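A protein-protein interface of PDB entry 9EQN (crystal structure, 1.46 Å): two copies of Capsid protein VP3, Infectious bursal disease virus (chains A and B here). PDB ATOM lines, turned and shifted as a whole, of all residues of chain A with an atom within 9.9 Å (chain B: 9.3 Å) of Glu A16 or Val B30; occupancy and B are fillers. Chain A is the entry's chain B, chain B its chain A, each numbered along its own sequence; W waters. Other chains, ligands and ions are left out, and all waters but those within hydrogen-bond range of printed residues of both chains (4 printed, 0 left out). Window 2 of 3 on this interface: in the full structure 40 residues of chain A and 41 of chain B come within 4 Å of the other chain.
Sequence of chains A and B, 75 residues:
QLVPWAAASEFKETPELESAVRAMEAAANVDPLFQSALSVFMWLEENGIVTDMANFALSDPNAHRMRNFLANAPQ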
ATOM      1  N   GLU A  10       4.091  26.483 -10.704  1.00  0.00           N
ATOM      2  CA  GLU A  10       3.153  25.415 -10.408  1.00  0.00           C
ATOM      3  C   GLU A  10       2.103  25.383 -11.506  1.00  0.00           C
ATOM      4  O   GLU A  10       1.776  26.415 -12.095  1.00  0.00           O
ATOM      5  CB  GLU A  10       2.450  25.716  -9.086  1.00  0.00           C
ATOM      6  CG  GLU A  10       1.881  24.534  -8.354  1.00  0.00           C
ATOM      7  CD  GLU A  10       0.606  24.883  -7.613  1.00  0.00           C
ATOM      8  OE1 GLU A  10       0.519  26.002  -7.065  1.00  0.00           O
ATOM      9  OE2 GLU A  10      -0.314  24.042  -7.590  1.00  0.00           O
ATOM     10  N   PHE A  11       1.578  24.191 -11.777  1.00  0.00           N
ATOM     11  CA  PHE A  11       0.499  24.069 -12.749  1.00  0.00           C
ATOM     12  C   PHE A  11      -0.708  24.887 -12.296  1.00  0.00           C
ATOM     13  O   PHE A  11      -1.055  24.915 -11.111  1.00  0.00           O
ATOM     14  CB  PHE A  11       0.088  22.603 -12.911  1.00  0.00           C
ATOM     15  CG  PHE A  11       1.139  21.736 -13.562  1.00  0.00           C
ATOM     16  CD1 PHE A  11       1.895  22.211 -14.631  1.00  0.00           C
ATOM     17  CD2 PHE A  11       1.370  20.443 -13.103  1.00  0.00           C
ATOM     18  CE1 PHE A  11       2.860  21.404 -15.243  1.00  0.00           C
ATOM     19  CE2 PHE A  11       2.332  19.629 -13.692  1.00  0.00           C
ATOM     20  CZ  PHE A  11       3.086  20.110 -14.758  1.00  0.00           C
ATOM     21  N   LYS A  12      -1.329  25.579 -13.247  1.00  0.00           N
ATOM     22  CA  LYS A  12      -2.564  26.303 -12.982  1.00  0.00           C
ATOM     23  C   LYS A  12      -3.660  25.313 -12.608  1.00  0.00           C
ATOM     24  O   LYS A  12      -3.798  24.255 -13.226  1.00  0.00           O
ATOM     25  CB  LYS A  12      -2.958  27.079 -14.243  1.00  0.00           C
ATOM     26  CG  LYS A  12      -4.195  27.951 -14.125  1.00  0.00           C
ATOM     27  CD  LYS A  12      -4.273  28.937 -15.295  1.00  0.00           C
ATOM     28  CE  LYS A  12      -5.421  29.925 -15.131  1.00  0.00           C
ATOM     29  NZ  LYS A  12      -6.196  30.104 -16.398  1.00  0.00           N
ATOM     30  N   GLU A  13      -4.434  25.640 -11.579  1.00  0.00           N
ATOM     31  CA  GLU A  13      -5.460  24.712 -11.097  1.00  0.00           C
ATOM     32  C   GLU A  13      -6.756  24.914 -11.875  1.00  0.00           C
ATOM     33  O   GLU A  13      -7.694  25.570 -11.426  1.00  0.00           O
ATOM     34  CB  GLU A  13      -5.600  24.772  -9.578  1.00  0.00           C
ATOM     35  CG  GLU A  13      -4.472  23.973  -8.927  1.00  0.00           C
ATOM     36  CD  GLU A  13      -4.379  24.122  -7.427  1.00  0.00           C
ATOM     37  OE1 GLU A  13      -5.033  25.026  -6.870  1.00  0.00           O
ATOM     38  OE2 GLU A  13      -3.634  23.334  -6.804  1.00  0.00           O
ATOM     39  N   THR A  14      -6.788  24.332 -13.059  1.00  0.00           N
ATOM     40  CA  THR A  14      -7.907  24.341 -13.981  1.00  0.00           C
ATOM     41  C   THR A  14      -8.651  23.020 -13.892  1.00  0.00           C
ATOM     42  O   THR A  14      -8.133  22.035 -13.356  1.00  0.00           O
ATOM     43  CB  THR A  14      -7.348  24.472 -15.402  1.00  0.00           C
ATOM     44  OG1 THR A  14      -6.538  23.324 -15.690  1.00  0.00           O
ATOM     45  CG2 THR A  14      -6.491  25.726 -15.526  1.00  0.00           C
ATOM     46  N   PRO A  15      -9.883  22.960 -14.393  1.00  0.00           N
ATOM     47  CA  PRO A  15     -10.536  21.650 -14.514  1.00  0.00           C
ATOM     48  C   PRO A  15      -9.779  20.721 -15.441  1.00  0.00           C
ATOM     49  O   PRO A  15      -9.758  19.505 -15.207  1.00  0.00           O
ATOM     50  CB  PRO A  15     -11.927  22.001 -15.067  1.00  0.00           C
ATOM     51  CG  PRO A  15     -12.122  23.457 -14.708  1.00  0.00           C
ATOM     52  CD  PRO A  15     -10.754  24.054 -14.854  1.00  0.00           C
ATOM     53  N   GLU A  16      -9.122  21.268 -16.471  1.00  0.00           N
ATOM     54  CA  GLU A  16      -8.341  20.435 -17.383  1.00  0.00           C
ATOM     55  C   GLU A  16      -7.179  19.768 -16.666  1.00  0.00           C
ATOM     56  O   GLU A  16      -6.827  18.626 -16.978  1.00  0.00           O
ATOM     57  CB  GLU A  16      -7.818  21.264 -18.560  1.00  0.00           C
ATOM     58  CG  GLU A  16      -8.857  21.548 -19.628  1.00  0.00           C
ATOM     59  CD  GLU A  16      -9.684  22.792 -19.357  1.00  0.00           C
ATOM     60  OE1 GLU A  16      -9.568  23.376 -18.262  1.00  0.00           O
ATOM     61  OE2 GLU A  16     -10.463  23.190 -20.254  1.00  0.00           O
ATOM     62  N   LEU A  17      -6.555  20.469 -15.718  1.00  0.00           N
ATOM     63  CA  LEU A  17      -5.460  19.864 -14.966  1.00  0.00           C
ATOM     64  C   LEU A  17      -5.940  18.651 -14.182  1.00  0.00           C
ATOM     65  O   LEU A  17      -5.331  17.572 -14.245  1.00  0.00           O
ATOM     66  CB  LEU A  17      -4.843  20.884 -14.008  1.00  0.00           C
ATOM     67  CG  LEU A  17      -3.787  20.264 -13.080  1.00  0.00           C
ATOM     68  CD1 LEU A  17      -2.586  19.782 -13.885  1.00  0.00           C
ATOM     69  CD2 LEU A  17      -3.364  21.233 -11.982  1.00  0.00           C
ATOM     70  N   GLU A  18      -7.036  18.813 -13.437  1.00  0.00           N
ATOM     71  CA  GLU A  18      -7.544  17.707 -12.634  1.00  0.00           C
ATOM     72  C   GLU A  18      -7.935  16.535 -13.518  1.00  0.00           C
ATOM     73  O   GLU A  18      -7.663  15.379 -13.182  1.00  0.00           O
ATOM     74  CB  GLU A  18      -8.715  18.170 -11.768  1.00  0.00           C
ATOM     75  CG  GLU A  18      -8.359  19.310 -10.811  1.00  0.00           C
ATOM     76  CD  GLU A  18      -7.389  18.901  -9.712  1.00  0.00           C
ATOM     77  OE1 GLU A  18      -7.783  18.094  -8.845  1.00  0.00           O
ATOM     78  OE2 GLU A  18      -6.236  19.391  -9.708  1.00  0.00           O
ATOM     79  N   SER A  19      -8.544  16.822 -14.670  1.00  0.00           N
ATOM     80  CA  SER A  19      -8.872  15.771 -15.623  1.00  0.00           C
ATOM     81  C   SER A  19      -7.614  15.121 -16.185  1.00  0.00           C
ATOM     82  O   SER A  19      -7.566  13.896 -16.359  1.00  0.00           O
ATOM     83  CB  SER A  19      -9.730  16.358 -16.743  1.00  0.00           C
ATOM     84  OG  SER A  19     -10.097  15.369 -17.684  1.00  0.00           O
ATOM     85  N   ALA A  20      -6.582  15.919 -16.475  1.00  0.00           N
ATOM     86  CA  ALA A  20      -5.353  15.351 -17.019  1.00  0.00           C
ATOM     87  C   ALA A  20      -4.627  14.506 -15.981  1.00  0.00           C
ATOM     88  O   ALA A  20      -4.111  13.432 -16.304  1.00  0.00           O
ATOM     89  CB  ALA A  20      -4.432  16.448 -17.550  1.00  0.00           C
ATOM     90  N   VAL A  21      -4.568  14.971 -14.734  1.00  0.00           N
ATOM     91  CA  VAL A  21      -3.911  14.189 -13.685  1.00  0.00           C
ATOM     92  C   VAL A  21      -4.610  12.848 -13.503  1.00  0.00           C
ATOM     93  O   VAL A  21      -3.968  11.792 -13.427  1.00  0.00           O
ATOM     94  CB  VAL A  21      -3.842  14.982 -12.366  1.00  0.00           C
ATOM     95  CG1 VAL A  21      -3.426  14.065 -11.208  1.00  0.00           C
ATOM     96  CG2 VAL A  21      -2.862  16.135 -12.500  1.00  0.00           C
ATOM     97  N   ARG A  22      -5.943  12.871 -13.435  1.00  0.00           N
ATOM     98  CA  ARG A  22      -6.667  11.624 -13.221  1.00  0.00           C
ATOM     99  C   ARG A  22      -6.518  10.685 -14.410  1.00  0.00           C
ATOM    100  O   ARG A  22      -6.398   9.472 -14.226  1.00  0.00           O
ATOM    101  CB  ARG A  22      -8.130  11.912 -12.863  1.00  0.00           C
ATOM    102  CG  ARG A  22      -8.339  12.059 -11.351  1.00  0.00           C
ATOM    103  CD  ARG A  22      -9.788  12.313 -10.981  1.00  0.00           C
ATOM    104  NE  ARG A  22     -10.424  13.271 -11.877  1.00  0.00           N
ATOM    105  CZ  ARG A  22     -10.731  14.519 -11.552  1.00  0.00           C
ATOM    106  NH1 ARG A  22     -10.482  15.002 -10.344  1.00  0.00           N
ATOM    107  NH2 ARG A  22     -11.309  15.301 -12.461  1.00  0.00           N
ATOM    108  N   ALA A  23      -6.480  11.233 -15.626  1.00  0.00           N
ATOM    109  CA  ALA A  23      -6.240  10.406 -16.806  1.00  0.00           C
ATOM    110  C   ALA A  23      -4.831   9.831 -16.801  1.00  0.00           C
ATOM    111  O   ALA A  23      -4.644   8.628 -17.024  1.00  0.00           O
ATOM    112  CB  ALA A  23      -6.495  11.206 -18.081  1.00  0.00           C
ATOM    113  N   MET A  24      -3.903  10.677 -16.446  1.00  0.00           N
ATOM    114  CA  MET A  24      -2.539  10.160 -16.418  1.00  0.00           C
ATOM    115  C   MET A  24      -2.368   9.098 -15.337  1.00  0.00           C
ATOM    116  O   MET A  24      -1.661   8.106 -15.546  1.00  0.00           O
ATOM    117  CB  MET A  24      -1.555  11.312 -16.201  1.00  0.00           C
ATOM    118  CG  MET A  24      -1.462  12.306 -17.358  1.00  0.00           C
ATOM    119  SD  MET A  24      -0.287  13.645 -17.031  1.00  0.00           S
ATOM    120  CE  MET A  24       1.291  12.875 -17.352  1.00  0.00           C
ATOM    121  N   PHE A  41       7.317  13.574 -14.851  1.00  0.00           N
ATOM    122  CA  PHE A  41       6.461  14.741 -15.050  1.00  0.00           C
ATOM    123  C   PHE A  41       6.194  15.448 -13.723  1.00  0.00           C
ATOM    124  O   PHE A  41       6.424  16.654 -13.591  1.00  0.00           O
ATOM    125  CB  PHE A  41       5.165  14.240 -15.686  1.00  0.00           C
ATOM    126  CG  PHE A  41       4.298  15.307 -16.297  1.00  0.00           C
ATOM    127  CD1 PHE A  41       4.453  15.674 -17.626  1.00  0.00           C
ATOM    128  CD2 PHE A  41       3.280  15.885 -15.573  1.00  0.00           C
ATOM    129  CE1 PHE A  41       3.629  16.626 -18.194  1.00  0.00           C
ATOM    130  CE2 PHE A  41       2.448  16.842 -16.135  1.00  0.00           C
ATOM    131  CZ  PHE A  41       2.626  17.212 -17.448  1.00  0.00           C
ATOM    132  N   SER B  19      -7.085   8.449 -23.749  1.00  0.00           N
ATOM    133  CA  SER B  19      -7.695   9.514 -22.954  1.00  0.00           C
ATOM    134  C   SER B  19      -6.638  10.414 -22.313  1.00  0.00           C
ATOM    135  O   SER B  19      -6.803  11.637 -22.259  1.00  0.00           O
ATOM    136  CB  SER B  19      -8.602   8.912 -21.883  1.00  0.00           C
ATOM    137  OG  SER B  19      -9.576   8.062 -22.454  1.00  0.00           O
ATOM    138  N   ALA B  20      -5.508   9.894 -21.839  1.00  0.00           N
ATOM    139  CA  ALA B  20      -4.488  10.680 -21.150  1.00  0.00           C
ATOM    140  C   ALA B  20      -3.873  11.717 -22.082  1.00  0.00           C
ATOM    141  O   ALA B  20      -3.771  12.902 -21.743  1.00  0.00           O
ATOM    142  CB  ALA B  20      -3.406   9.756 -20.596  1.00  0.00           C
ATOM    143  N   ARG B  22      -5.018  13.000 -24.926  1.00  0.00           N
ATOM    144  CA  ARG B  22      -6.059  13.997 -25.168  1.00  0.00           C
ATOM    145  C   ARG B  22      -6.183  14.956 -23.990  1.00  0.00           C
ATOM    146  O   ARG B  22      -6.307  16.172 -24.179  1.00  0.00           O
ATOM    147  CB  ARG B  22      -7.399  13.316 -25.457  1.00  0.00           C
ATOM    148  CG  ARG B  22      -7.371  12.400 -26.666  1.00  0.00           C
ATOM    149  CD  ARG B  22      -8.706  11.691 -26.886  1.00  0.00           C
ATOM    150  NE  ARG B  22      -9.794  12.621 -27.149  1.00  0.00           N
ATOM    151  CZ  ARG B  22     -10.788  12.880 -26.305  1.00  0.00           C
ATOM    152  NH1 ARG B  22     -10.868  12.284 -25.126  1.00  0.00           N
ATOM    153  NH2 ARG B  22     -11.730  13.752 -26.657  1.00  0.00           N
ATOM    154  N   ALA B  23      -6.297  14.406 -22.864  1.00  0.00           N
ATOM    155  CA  ALA B  23      -6.492  15.280 -21.712  1.00  0.00           C
ATOM    156  C   ALA B  23      -5.277  16.169 -21.481  1.00  0.00           C
ATOM    157  O   ALA B  23      -5.424  17.341 -21.116  1.00  0.00           O
ATOM    158  CB  ALA B  23      -6.822  14.465 -20.463  1.00  0.00           C
ATOM    159  N   MET B  24      -4.113  15.688 -21.639  1.00  0.00           N
ATOM    160  CA  MET B  24      -2.882  16.465 -21.518  1.00  0.00           C
ATOM    161  C   MET B  24      -2.831  17.602 -22.530  1.00  0.00           C
ATOM    162  O   MET B  24      -2.419  18.720 -22.198  1.00  0.00           O
ATOM    163  CB  MET B  24      -1.666  15.560 -21.701  1.00  0.00           C
ATOM    164  CG  MET B  24      -1.455  14.564 -20.571  1.00  0.00           C
ATOM    165  SD  MET B  24      -0.100  13.414 -20.850  1.00  0.00           S
ATOM    166  CE  MET B  24       1.355  14.363 -20.496  1.00  0.00           C
ATOM    167  N   GLU B  25      -3.192  17.330 -23.781  1.00  0.00           N
ATOM    168  CA  GLU B  25      -3.236  18.409 -24.766  1.00  0.00           C
ATOM    169  C   GLU B  25      -4.213  19.505 -24.343  1.00  0.00           C
ATOM    170  O   GLU B  25      -3.917  20.697 -24.479  1.00  0.00           O
ATOM    171  CB  GLU B  25      -3.618  17.854 -26.136  1.00  0.00           C
ATOM    172  CG  GLU B  25      -3.662  18.917 -27.206  1.00  0.00           C
ATOM    173  CD  GLU B  25      -3.842  18.348 -28.587  1.00  0.00           C
ATOM    174  OE1 GLU B  25      -4.239  17.168 -28.706  1.00  0.00           O
ATOM    175  OE2 GLU B  25      -3.583  19.091 -29.553  1.00  0.00           O
ATOM    176  N   ALA B  26      -5.376  19.119 -23.814  1.00  0.00           N
ATOM    177  CA  ALA B  26      -6.349  20.110 -23.361  1.00  0.00           C
ATOM    178  C   ALA B  26      -5.815  20.905 -22.169  1.00  0.00           C
ATOM    179  O   ALA B  26      -6.030  22.123 -22.074  1.00  0.00           O
ATOM    180  CB  ALA B  26      -7.672  19.429 -23.015  1.00  0.00           C
ATOM    181  N   ALA B  27      -5.128  20.237 -21.241  1.00  0.00           N
ATOM    182  CA  ALA B  27      -4.522  20.969 -20.133  1.00  0.00           C
ATOM    183  C   ALA B  27      -3.431  21.909 -20.630  1.00  0.00           C
ATOM    184  O   ALA B  27      -3.296  23.034 -20.127  1.00  0.00           O
ATOM    185  CB  ALA B  27      -3.952  19.994 -19.105  1.00  0.00           C
ATOM    186  N   ALA B  28      -2.649  21.466 -21.624  1.00  0.00           N
ATOM    187  CA  ALA B  28      -1.582  22.302 -22.171  1.00  0.00           C
ATOM    188  C   ALA B  28      -2.134  23.527 -22.879  1.00  0.00           C
ATOM    189  O   ALA B  28      -1.485  24.578 -22.899  1.00  0.00           O
ATOM    190  CB  ALA B  28      -0.724  21.505 -23.159  1.00  0.00           C
ATOM    191  N   ASN B  29      -3.313  23.407 -23.488  1.00  0.00           N
ATOM    192  CA  ASN B  29      -3.901  24.543 -24.186  1.00  0.00           C
ATOM    193  C   ASN B  29      -4.213  25.682 -23.225  1.00  0.00           C
ATOM    194  O   ASN B  29      -4.011  26.855 -23.558  1.00  0.00           O
ATOM    195  CB  ASN B  29      -5.164  24.087 -24.913  1.00  0.00           C
ATOM    196  CG  ASN B  29      -5.687  25.125 -25.868  1.00  0.00           C
ATOM    197  OD1 ASN B  29      -5.448  25.048 -27.073  1.00  0.00           O
ATOM    198  ND2 ASN B  29      -6.410  26.105 -25.342  1.00  0.00           N
ATOM    199  N   VAL B  30      -4.667  25.357 -22.010  1.00  0.00           N
ATOM    200  CA  VAL B  30      -5.085  26.370 -21.046  1.00  0.00           C
ATOM    201  C   VAL B  30      -4.000  26.721 -20.025  1.00  0.00           C
ATOM    202  O   VAL B  30      -4.206  27.660 -19.231  1.00  0.00           O
ATOM    203  CB  VAL B  30      -6.408  25.987 -20.344  1.00  0.00           C
ATOM    204  CG1 VAL B  30      -7.519  25.780 -21.369  1.00  0.00           C
ATOM    205  CG2 VAL B  30      -6.226  24.736 -19.480  1.00  0.00           C
ATOM    206  N   ASP B  31      -2.872  26.024 -20.015  1.00  0.00           N
ATOM    207  CA  ASP B  31      -1.779  26.317 -19.083  1.00  0.00           C
ATOM    208  C   ASP B  31      -0.453  26.096 -19.798  1.00  0.00           C
ATOM    209  O   ASP B  31      -0.025  24.945 -19.982  1.00  0.00           O
ATOM    210  CB  ASP B  31      -1.842  25.451 -17.826  1.00  0.00           C
ATOM    211  CG  ASP B  31      -0.707  25.741 -16.854  1.00  0.00           C
ATOM    212  OD1 ASP B  31       0.016  26.750 -17.049  1.00  0.00           O
ATOM    213  OD2 ASP B  31      -0.533  24.964 -15.896  1.00  0.00           O
ATOM    214  N   PRO B  32       0.244  27.165 -20.178  1.00  0.00           N
ATOM    215  CA  PRO B  32       1.536  26.988 -20.859  1.00  0.00           C
ATOM    216  C   PRO B  32       2.586  26.250 -20.049  1.00  0.00           C
ATOM    217  O   PRO B  32       3.471  25.632 -20.655  1.00  0.00           O
ATOM    218  CB  PRO B  32       1.980  28.422 -21.195  1.00  0.00           C
ATOM    219  CG  PRO B  32       1.087  29.324 -20.420  1.00  0.00           C
ATOM    220  CD  PRO B  32      -0.167  28.577 -20.093  1.00  0.00           C
ATOM    221  N   LEU B  33       2.543  26.283 -18.713  1.00  0.00           N
ATOM    222  CA  LEU B  33       3.488  25.456 -17.966  1.00  0.00           C
ATOM    223  C   LEU B  33       3.216  23.972 -18.185  1.00  0.00           C
ATOM    224  O   LEU B  33       4.149  23.177 -18.329  1.00  0.00           O
ATOM    225  CB  LEU B  33       3.446  25.801 -16.473  1.00  0.00           C
ATOM    226  CG  LEU B  33       4.541  25.135 -15.637  1.00  0.00           C
ATOM    227  CD1 LEU B  33       5.926  25.665 -16.006  1.00  0.00           C
ATOM    228  CD2 LEU B  33       4.261  25.342 -14.161  1.00  0.00           C
ATOM    229  N   PHE B  34       1.947  23.581 -18.218  1.00  0.00           N
ATOM    230  CA  PHE B  34       1.637  22.205 -18.585  1.00  0.00           C
ATOM    231  C   PHE B  34       2.085  21.906 -20.014  1.00  0.00           C
ATOM    232  O   PHE B  34       2.578  20.810 -20.292  1.00  0.00           O
ATOM    233  CB  PHE B  34       0.141  21.957 -18.401  1.00  0.00           C
ATOM    234  CG  PHE B  34      -0.222  20.514 -18.268  1.00  0.00           C
ATOM    235  CD1 PHE B  34      -0.296  19.696 -19.387  1.00  0.00           C
ATOM    236  CD2 PHE B  34      -0.494  19.968 -17.019  1.00  0.00           C
ATOM    237  CE1 PHE B  34      -0.623  18.359 -19.266  1.00  0.00           C
ATOM    238  CE2 PHE B  34      -0.831  18.629 -16.884  1.00  0.00           C
ATOM    239  CZ  PHE B  34      -0.895  17.822 -18.008  1.00  0.00           C
ATOM    240  N   GLN B  35       1.976  22.876 -20.893  1.00  0.00           N
ATOM    241  CA  GLN B  35       2.478  22.677 -22.265  1.00  0.00           C
ATOM    242  C   GLN B  35       4.004  22.462 -22.262  1.00  0.00           C
ATOM    243  O   GLN B  35       4.481  21.620 -23.022  1.00  0.00           O
ATOM    244  CB  GLN B  35       2.101  23.902 -23.105  1.00  0.00           C
ATOM    245  CG  GLN B  35       2.326  23.651 -24.584  1.00  0.00           C
ATOM    246  CD  GLN B  35       1.573  24.650 -25.416  1.00  0.00           C
ATOM    247  OE1 GLN B  35       1.835  25.843 -25.354  1.00  0.00           O
ATOM    248  NE2 GLN B  35       0.641  24.154 -26.208  1.00  0.00           N
HETATM  249  O   HOH W   1      -2.450  23.200 -15.370  1.00  0.00           O
HETATM  250  O   HOH W   2       1.092  27.596 -14.489  1.00  0.00           O
HETATM  251  O   HOH W   3      -4.468  23.083 -17.308  1.00  0.00           O
HETATM  252  O   HOH W   4      -7.667  18.041 -19.494  1.00  0.00           O
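Glu A16 touches three residues of chain B. Of chain A, only Glu A16 (3.7 Å) and Ala A20 (3.9 Å) come within 4 Å of Ala B27. Ala B28 touches none of the printed residues of chain A. No residue of chain A comes within 4 Å of Asn B29. Asp B31 touches just these residues of chain A: Phe A11 (3.4 Å) and Lys A12 (2.8 Å). Printed residues of chain B within 4 Å of Glu A10: Leu B33. Printed residues of chain A within 4 Å of Ala B26: Glu A16. Printed residues of chain B within 4 Å of Ala A23: Ala B20. Of the printed residues of chain A, Ala B20 touches Ala A23 (3.7 Å). Glu A13 touches none of the printed residues of chain B. Glu A18 touches none of the printed residues of chain B. The nearest residue of chain B that does not touch Glu A16 is Ala B23 (4.6 Å).
Among the printed residues, merely in contact across the chains: Glu A10 with Leu B33 (3.4 Å), Phe A11 with Asp B31 (3.4 Å), Phe A11 with Leu B33 (3.8 Å), Phe A11 with Phe B34 (3.6 Å), Glu A16 with Ala B26 (3.8 Å), Glu A16 with Ala B27 (3.7 Å), Glu A16 with Val B30 (3.8 Å), Leu A17 with Phe B34 (3.7 Å), Ala A20 with Ala B23 (3.8 Å), Ala A20 with Ala B27 (3.9 Å), Ala A20 with Phe B34 (3.8 Å), Ala A23 with Ala B20 (3.7 Å), Met A24 with Met B24 (3.5 Å), Phe A41 with Met B24 (3.9 Å) and Phe A41 with Phe B34 (3.6 Å).
Hydrophobic or aromatic side chains of chain A that line the printed part of chain B: Phe A11, Leu A17, Ala A20, Ala A23, Met A24 and Phe A41. Of the 16 printed residues of chain B, 9 touch a printed residue of chain A. Hydrophobic or aromatic side chains of chain B that line the printed part of chain A: Ala B20, Ala B23, Met B24, Ala B27, Val B30, Leu B33 and Phe B34. Along chain B the printed residues that touch a printed residue of chain A span positions 20 to 34. Among the printed residues, 16 pairs touch across the chains. Among the printed residues, no Asp or Glu carboxylate lies within 4 Å of a Lys or Arg side-chain nitrogen of the other chain.
OD2 of Asp B31 sits at hydrogen-bond distance from N of Lys A12.
Ala A20 touches Ala B23, and with the chains exchanged Ala A23 touches Ala B20. Met A24 touches its own counterpart, Met B24. 5 positions are printed for both chains.
Water W3 bridges the side-chain hydroxyl of Thr A14 (2.6 Å) and the backbone carbonyl oxygen of Ala B27 (3.1 Å). Water W1 bridges OD2 of Asp B31 and O of Lys A12. Water W4 bridges the backbone carbonyl oxygen (O) of Glu A16 (2.7 Å) and the backbone carbonyl oxygen (O) of Ala B23 (2.9 Å). Water W2 lies within hydrogen-bond range of O of Glu A10 (2.8 Å), OD1 of Asp B31 (2.9 Å) and N of Lys A12 (3.4 Å).
The side-chain carboxylate of Asp B31 sits at hydrogen-bond distance from the backbone NH of Leu B33, at 3.1 Å. The side-chain hydroxyl of Thr A14 sits close to the backbone NH of Glu A16 (3.4 Å). The side-chain hydroxyl (OG1) of Thr A14 lies within hydrogen-bond range of the backbone NH (N) of Leu A17, at 2.9 Å.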
